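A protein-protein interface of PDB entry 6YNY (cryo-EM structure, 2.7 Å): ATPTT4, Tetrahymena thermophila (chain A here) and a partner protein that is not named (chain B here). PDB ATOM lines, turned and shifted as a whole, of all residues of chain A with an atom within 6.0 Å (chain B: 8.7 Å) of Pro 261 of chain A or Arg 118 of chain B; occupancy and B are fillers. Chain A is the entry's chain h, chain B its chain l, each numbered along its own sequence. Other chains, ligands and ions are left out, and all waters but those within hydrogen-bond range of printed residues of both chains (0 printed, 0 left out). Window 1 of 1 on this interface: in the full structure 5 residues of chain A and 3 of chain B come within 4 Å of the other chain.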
ATOM      1  N   ARG A 255     -14.651   8.485   3.959  1.00  0.00           N
ATOM      2  CA  ARG A 255     -15.910   8.559   3.240  1.00  0.00           C
ATOM      3  C   ARG A 255     -15.673   9.211   1.887  1.00  0.00           C
ATOM      4  O   ARG A 255     -14.755  10.017   1.723  1.00  0.00           O
ATOM      5  CB  ARG A 255     -16.946   9.355   4.037  1.00  0.00           C
ATOM      6  CG  ARG A 255     -18.349   9.288   3.481  1.00  0.00           C
ATOM      7  CD  ARG A 255     -19.100  10.578   3.704  1.00  0.00           C
ATOM      8  NE  ARG A 255     -19.880  10.586   4.933  1.00  0.00           N
ATOM      9  CZ  ARG A 255     -21.170  10.282   5.003  1.00  0.00           C
ATOM     10  NH1 ARG A 255     -21.845   9.937   3.917  1.00  0.00           N
ATOM     11  NH2 ARG A 255     -21.792  10.326   6.167  1.00  0.00           N
ATOM     12  N   ARG A 256     -16.498   8.841   0.914  1.00  0.00           N
ATOM     13  CA  ARG A 256     -16.421   9.467  -0.390  1.00  0.00           C
ATOM     14  C   ARG A 256     -16.745  10.954  -0.268  1.00  0.00           C
ATOM     15  O   ARG A 256     -17.573  11.349   0.558  1.00  0.00           O
ATOM     16  CB  ARG A 256     -17.387   8.815  -1.370  1.00  0.00           C
ATOM     17  CG  ARG A 256     -17.044   7.404  -1.765  1.00  0.00           C
ATOM     18  CD  ARG A 256     -17.904   6.966  -2.925  1.00  0.00           C
ATOM     19  NE  ARG A 256     -17.641   5.596  -3.348  1.00  0.00           N
ATOM     20  CZ  ARG A 256     -16.698   5.245  -4.213  1.00  0.00           C
ATOM     21  NH1 ARG A 256     -15.903   6.155  -4.754  1.00  0.00           N
ATOM     22  NH2 ARG A 256     -16.549   3.973  -4.534  1.00  0.00           N
ATOM     23  N   PRO A 257     -16.111  11.800  -1.071  1.00  0.00           N
ATOM     24  CA  PRO A 257     -16.431  13.225  -1.020  1.00  0.00           C
ATOM     25  C   PRO A 257     -17.816  13.505  -1.575  1.00  0.00           C
ATOM     26  O   PRO A 257     -18.336  12.770  -2.417  1.00  0.00           O
ATOM     27  CB  PRO A 257     -15.343  13.863  -1.887  1.00  0.00           C
ATOM     28  CG  PRO A 257     -14.924  12.806  -2.792  1.00  0.00           C
ATOM     29  CD  PRO A 257     -15.053  11.519  -2.052  1.00  0.00           C
ATOM     30  N   PHE A 258     -18.414  14.589  -1.083  1.00  0.00           N
ATOM     31  CA  PHE A 258     -19.752  14.957  -1.523  1.00  0.00           C
ATOM     32  C   PHE A 258     -19.819  15.119  -3.033  1.00  0.00           C
ATOM     33  O   PHE A 258     -20.852  14.823  -3.645  1.00  0.00           O
ATOM     34  CB  PHE A 258     -20.177  16.244  -0.824  1.00  0.00           C
ATOM     35  CG  PHE A 258     -21.595  16.642  -1.085  1.00  0.00           C
ATOM     36  CD1 PHE A 258     -22.619  16.156  -0.297  1.00  0.00           C
ATOM     37  CD2 PHE A 258     -21.904  17.515  -2.107  1.00  0.00           C
ATOM     38  CE1 PHE A 258     -23.919  16.524  -0.532  1.00  0.00           C
ATOM     39  CE2 PHE A 258     -23.202  17.884  -2.344  1.00  0.00           C
ATOM     40  CZ  PHE A 258     -24.211  17.390  -1.555  1.00  0.00           C
ATOM     41  N   GLU A 259     -18.737  15.582  -3.652  1.00  0.00           N
ATOM     42  CA  GLU A 259     -18.741  15.896  -5.071  1.00  0.00           C
ATOM     43  C   GLU A 259     -18.458  14.686  -5.948  1.00  0.00           C
ATOM     44  O   GLU A 259     -18.551  14.795  -7.175  1.00  0.00           O
ATOM     45  CB  GLU A 259     -17.717  16.989  -5.379  1.00  0.00           C
ATOM     46  CG  GLU A 259     -17.997  18.314  -4.703  1.00  0.00           C
ATOM     47  CD  GLU A 259     -17.656  18.310  -3.227  1.00  0.00           C
ATOM     48  OE1 GLU A 259     -17.308  17.235  -2.699  1.00  0.00           O
ATOM     49  OE2 GLU A 259     -17.732  19.385  -2.598  1.00  0.00           O
ATOM     50  N   HIS A 260     -18.092  13.550  -5.361  1.00  0.00           N
ATOM     51  CA  HIS A 260     -17.843  12.319  -6.109  1.00  0.00           C
ATOM     52  C   HIS A 260     -18.388  11.147  -5.312  1.00  0.00           C
ATOM     53  O   HIS A 260     -17.653  10.474  -4.580  1.00  0.00           O
ATOM     54  CB  HIS A 260     -16.354  12.133  -6.396  1.00  0.00           C
ATOM     55  CG  HIS A 260     -15.723  13.288  -7.103  1.00  0.00           C
ATOM     56  ND1 HIS A 260     -15.544  13.317  -8.468  1.00  0.00           N
ATOM     57  CD2 HIS A 260     -15.217  14.452  -6.633  1.00  0.00           C
ATOM     58  CE1 HIS A 260     -14.962  14.451  -8.810  1.00  0.00           C
ATOM     59  NE2 HIS A 260     -14.752  15.158  -7.715  1.00  0.00           N
ATOM     60  N   PRO A 261     -19.674  10.867  -5.435  1.00  0.00           N
ATOM     61  CA  PRO A 261     -20.232   9.683  -4.778  1.00  0.00           C
ATOM     62  C   PRO A 261     -20.073   8.427  -5.613  1.00  0.00           C
ATOM     63  O   PRO A 261     -19.586   8.480  -6.745  1.00  0.00           O
ATOM     64  CB  PRO A 261     -21.707  10.056  -4.605  1.00  0.00           C
ATOM     65  CG  PRO A 261     -21.980  10.961  -5.725  1.00  0.00           C
ATOM     66  CD  PRO A 261     -20.730  11.754  -5.942  1.00  0.00           C
ATOM     67  N   ASN A 262     -20.484   7.298  -5.063  1.00  0.00           N
ATOM     68  CA  ASN A 262     -20.401   6.032  -5.768  1.00  0.00           C
ATOM     69  C   ASN A 262     -21.331   6.063  -6.971  1.00  0.00           C
ATOM     70  O   ASN A 262     -22.554   6.027  -6.788  1.00  0.00           O
ATOM     71  CB  ASN A 262     -20.771   4.879  -4.848  1.00  0.00           C
ATOM     72  CG  ASN A 262     -20.517   3.531  -5.481  1.00  0.00           C
ATOM     73  OD1 ASN A 262     -19.916   3.438  -6.549  1.00  0.00           O
ATOM     74  ND2 ASN A 262     -20.968   2.476  -4.824  1.00  0.00           N
ATOM     75  N   PRO A 263     -20.820   6.138  -8.202  1.00  0.00           N
ATOM     76  CA  PRO A 263     -21.727   6.257  -9.347  1.00  0.00           C
ATOM     77  C   PRO A 263     -22.299   4.932  -9.802  1.00  0.00           C
ATOM     78  O   PRO A 263     -23.299   4.929 -10.531  1.00  0.00           O
ATOM     79  CB  PRO A 263     -20.830   6.864 -10.427  1.00  0.00           C
ATOM     80  CG  PRO A 263     -19.482   6.305 -10.116  1.00  0.00           C
ATOM     81  CD  PRO A 263     -19.413   6.073  -8.630  1.00  0.00           C
ATOM     82  N   THR A 264     -21.692   3.817  -9.410  1.00  0.00           N
ATOM     83  CA  THR A 264     -22.012   2.525  -9.995  1.00  0.00           C
ATOM     84  C   THR A 264     -23.064   1.752  -9.215  1.00  0.00           C
ATOM     85  O   THR A 264     -23.739   0.898  -9.798  1.00  0.00           O
ATOM     86  CB  THR A 264     -20.745   1.678 -10.106  1.00  0.00           C
ATOM     87  OG1 THR A 264     -20.121   1.576  -8.821  1.00  0.00           O
ATOM     88  CG2 THR A 264     -19.782   2.304 -11.096  1.00  0.00           C
ATOM     89  N   LEU B 115     -31.379  14.012 -13.168  1.00  0.00           N
ATOM     90  CA  LEU B 115     -31.516  14.912 -12.034  1.00  0.00           C
ATOM     91  C   LEU B 115     -30.265  14.862 -11.163  1.00  0.00           C
ATOM     92  O   LEU B 115     -29.799  13.767 -10.822  1.00  0.00           O
ATOM     93  CB  LEU B 115     -32.736  14.552 -11.193  1.00  0.00           C
ATOM     94  CG  LEU B 115     -33.976  15.424 -11.351  1.00  0.00           C
ATOM     95  CD1 LEU B 115     -35.027  14.975 -10.363  1.00  0.00           C
ATOM     96  CD2 LEU B 115     -33.652  16.884 -11.144  1.00  0.00           C
ATOM     97  N   PRO B 116     -29.705  16.008 -10.767  1.00  0.00           N
ATOM     98  CA  PRO B 116     -28.501  15.986  -9.926  1.00  0.00           C
ATOM     99  C   PRO B 116     -28.767  15.686  -8.460  1.00  0.00           C
ATOM    100  O   PRO B 116     -27.913  15.952  -7.613  1.00  0.00           O
ATOM    101  CB  PRO B 116     -27.930  17.400 -10.095  1.00  0.00           C
ATOM    102  CG  PRO B 116     -28.642  17.989 -11.230  1.00  0.00           C
ATOM    103  CD  PRO B 116     -29.974  17.364 -11.266  1.00  0.00           C
ATOM    104  N   LEU B 117     -29.942  15.172  -8.128  1.00  0.00           N
ATOM    105  CA  LEU B 117     -30.192  14.775  -6.750  1.00  0.00           C
ATOM    106  C   LEU B 117     -29.198  13.702  -6.337  1.00  0.00           C
ATOM    107  O   LEU B 117     -29.117  12.641  -6.963  1.00  0.00           O
ATOM    108  CB  LEU B 117     -31.621  14.277  -6.582  1.00  0.00           C
ATOM    109  CG  LEU B 117     -32.721  15.300  -6.837  1.00  0.00           C
ATOM    110  CD1 LEU B 117     -34.052  14.730  -6.435  1.00  0.00           C
ATOM    111  CD2 LEU B 117     -32.449  16.580  -6.091  1.00  0.00           C
ATOM    112  N   ARG B 118     -28.434  13.984  -5.282  1.00  0.00           N
ATOM    113  CA  ARG B 118     -27.380  13.068  -4.867  1.00  0.00           C
ATOM    114  C   ARG B 118     -27.956  11.736  -4.407  1.00  0.00           C
ATOM    115  O   ARG B 118     -27.553  10.673  -4.890  1.00  0.00           O
ATOM    116  CB  ARG B 118     -26.549  13.706  -3.756  1.00  0.00           C
ATOM    117  CG  ARG B 118     -25.420  12.839  -3.261  1.00  0.00           C
ATOM    118  CD  ARG B 118     -24.749  13.432  -2.052  1.00  0.00           C
ATOM    119  NE  ARG B 118     -23.822  12.486  -1.440  1.00  0.00           N
ATOM    120  CZ  ARG B 118     -22.557  12.329  -1.810  1.00  0.00           C
ATOM    121  NH1 ARG B 118     -22.047  13.055  -2.790  1.00  0.00           N
ATOM    122  NH2 ARG B 118     -21.802  11.437  -1.195  1.00  0.00           N
ATOM    123  N   ASN B 119     -28.896  11.771  -3.468  1.00  0.00           N
ATOM    124  CA  ASN B 119     -29.410  10.539  -2.891  1.00  0.00           C
ATOM    125  C   ASN B 119     -30.196   9.747  -3.927  1.00  0.00           C
ATOM    126  O   ASN B 119     -31.092  10.278  -4.588  1.00  0.00           O
ATOM    127  CB  ASN B 119     -30.289  10.843  -1.684  1.00  0.00           C
ATOM    128  CG  ASN B 119     -30.631   9.603  -0.891  1.00  0.00           C
ATOM    129  OD1 ASN B 119     -30.778   8.516  -1.442  1.00  0.00           O
ATOM    130  ND2 ASN B 119     -30.755   9.761   0.414  1.00  0.00           N
ATOM    131  N   PHE B 120     -29.853   8.468  -4.060  1.00  0.00           N
ATOM    132  CA  PHE B 120     -30.548   7.599  -5.002  1.00  0.00           C
ATOM    133  C   PHE B 120     -32.017   7.448  -4.638  1.00  0.00           C
ATOM    134  O   PHE B 120     -32.887   7.469  -5.516  1.00  0.00           O
ATOM    135  CB  PHE B 120     -29.855   6.241  -5.041  1.00  0.00           C
ATOM    136  CG  PHE B 120     -30.650   5.168  -5.711  1.00  0.00           C
ATOM    137  CD1 PHE B 120     -30.902   5.215  -7.064  1.00  0.00           C
ATOM    138  CD2 PHE B 120     -31.126   4.098  -4.986  1.00  0.00           C
ATOM    139  CE1 PHE B 120     -31.626   4.224  -7.673  1.00  0.00           C
ATOM    140  CE2 PHE B 120     -31.850   3.107  -5.593  1.00  0.00           C
ATOM    141  CZ  PHE B 120     -32.098   3.168  -6.936  1.00  0.00           C
ATOM    142  N   TYR B 121     -32.317   7.311  -3.347  1.00  0.00           N
ATOM    143  CA  TYR B 121     -33.695   7.122  -2.921  1.00  0.00           C
ATOM    144  C   TYR B 121     -34.525   8.391  -3.044  1.00  0.00           C
ATOM    145  O   TYR B 121     -35.757   8.312  -3.033  1.00  0.00           O
ATOM    146  CB  TYR B 121     -33.720   6.602  -1.487  1.00  0.00           C
ATOM    147  CG  TYR B 121     -32.985   5.298  -1.327  1.00  0.00           C
ATOM    148  CD1 TYR B 121     -31.801   5.231  -0.617  1.00  0.00           C
ATOM    149  CD2 TYR B 121     -33.464   4.136  -1.908  1.00  0.00           C
ATOM    150  CE1 TYR B 121     -31.125   4.046  -0.477  1.00  0.00           C
ATOM    151  CE2 TYR B 121     -32.793   2.947  -1.772  1.00  0.00           C
ATOM    152  CZ  TYR B 121     -31.624   2.907  -1.057  1.00  0.00           C
ATOM    153  OH  TYR B 121     -30.949   1.721  -0.921  1.00  0.00           O
ATOM    154  N   ALA B 122     -33.884   9.552  -3.165  1.00  0.00           N
ATOM    155  CA  ALA B 122     -34.625  10.773  -3.454  1.00  0.00           C
ATOM    156  C   ALA B 122     -35.144  10.772  -4.884  1.00  0.00           C
ATOM    157  O   ALA B 122     -36.288  11.166  -5.137  1.00  0.00           O
ATOM    158  CB  ALA B 122     -33.739  11.989  -3.211  1.00  0.00           C
ATOM    159  N   ARG B 123     -34.317  10.333  -5.832  1.00  0.00           N
ATOM    160  CA  ARG B 123     -34.768  10.205  -7.211  1.00  0.00           C
ATOM    161  C   ARG B 123     -35.796   9.095  -7.366  1.00  0.00           C
ATOM    162  O   ARG B 123     -36.606   9.128  -8.298  1.00  0.00           O
ATOM    163  CB  ARG B 123     -33.571   9.956  -8.122  1.00  0.00           C
ATOM    164  CG  ARG B 123     -32.494  10.998  -7.982  1.00  0.00           C
ATOM    165  CD  ARG B 123     -31.485  10.945  -9.097  1.00  0.00           C
ATOM    166  NE  ARG B 123     -30.827   9.650  -9.209  1.00  0.00           N
ATOM    167  CZ  ARG B 123     -29.782   9.273  -8.487  1.00  0.00           C
ATOM    168  NH1 ARG B 123     -29.263  10.082  -7.581  1.00  0.00           N
ATOM    169  NH2 ARG B 123     -29.257   8.077  -8.672  1.00  0.00           N
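The guanidinium group (NH1) of Arg 118 of chain B sits close to the backbone carbonyl oxygen (O) of Phe 258 of chain A (2.3 Å).
The backbone carbonyl oxygen (O) of Arg 118 of chain B is in hydrogen-bond range of the guanidinium group (NH1) of Arg 123 of chain B (3.2 Å).
Among the printed residues, merely in contact across the chains: Pro 261 of chain A with Arg 118 of chain B (3.5 Å) and Pro 257 of chain A with Arg 118 of chain B (3.7 Å).
Of the 10 printed residues of chain A, 3 touch a printed residue of chain B.
Printed residues of chain A that touch a printed residue of chain B: Pro 257, Phe 258 and Pro 261.
Hydrophobic or aromatic side chains of chain A that line the printed part of chain B: Phe 258 and Pro 261.
Along chain A the printed residues that touch a printed residue of chain B span positions 257 to 261.
Among the printed residues, no Asp or Glu carboxylate lies within 4 Å of a Lys or Arg side-chain nitrogen of the other chain.
Of the printed residues of chain B, Pro 257 of chain A touches Arg 118.
Of the printed residues of chain B, Phe 258 of chain A touches Arg 118.
Pro 261 of chain A touches just one residue of chain B: Arg 118 (3.5 Å).
Arg 118 of chain B touches three residues of chain A.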
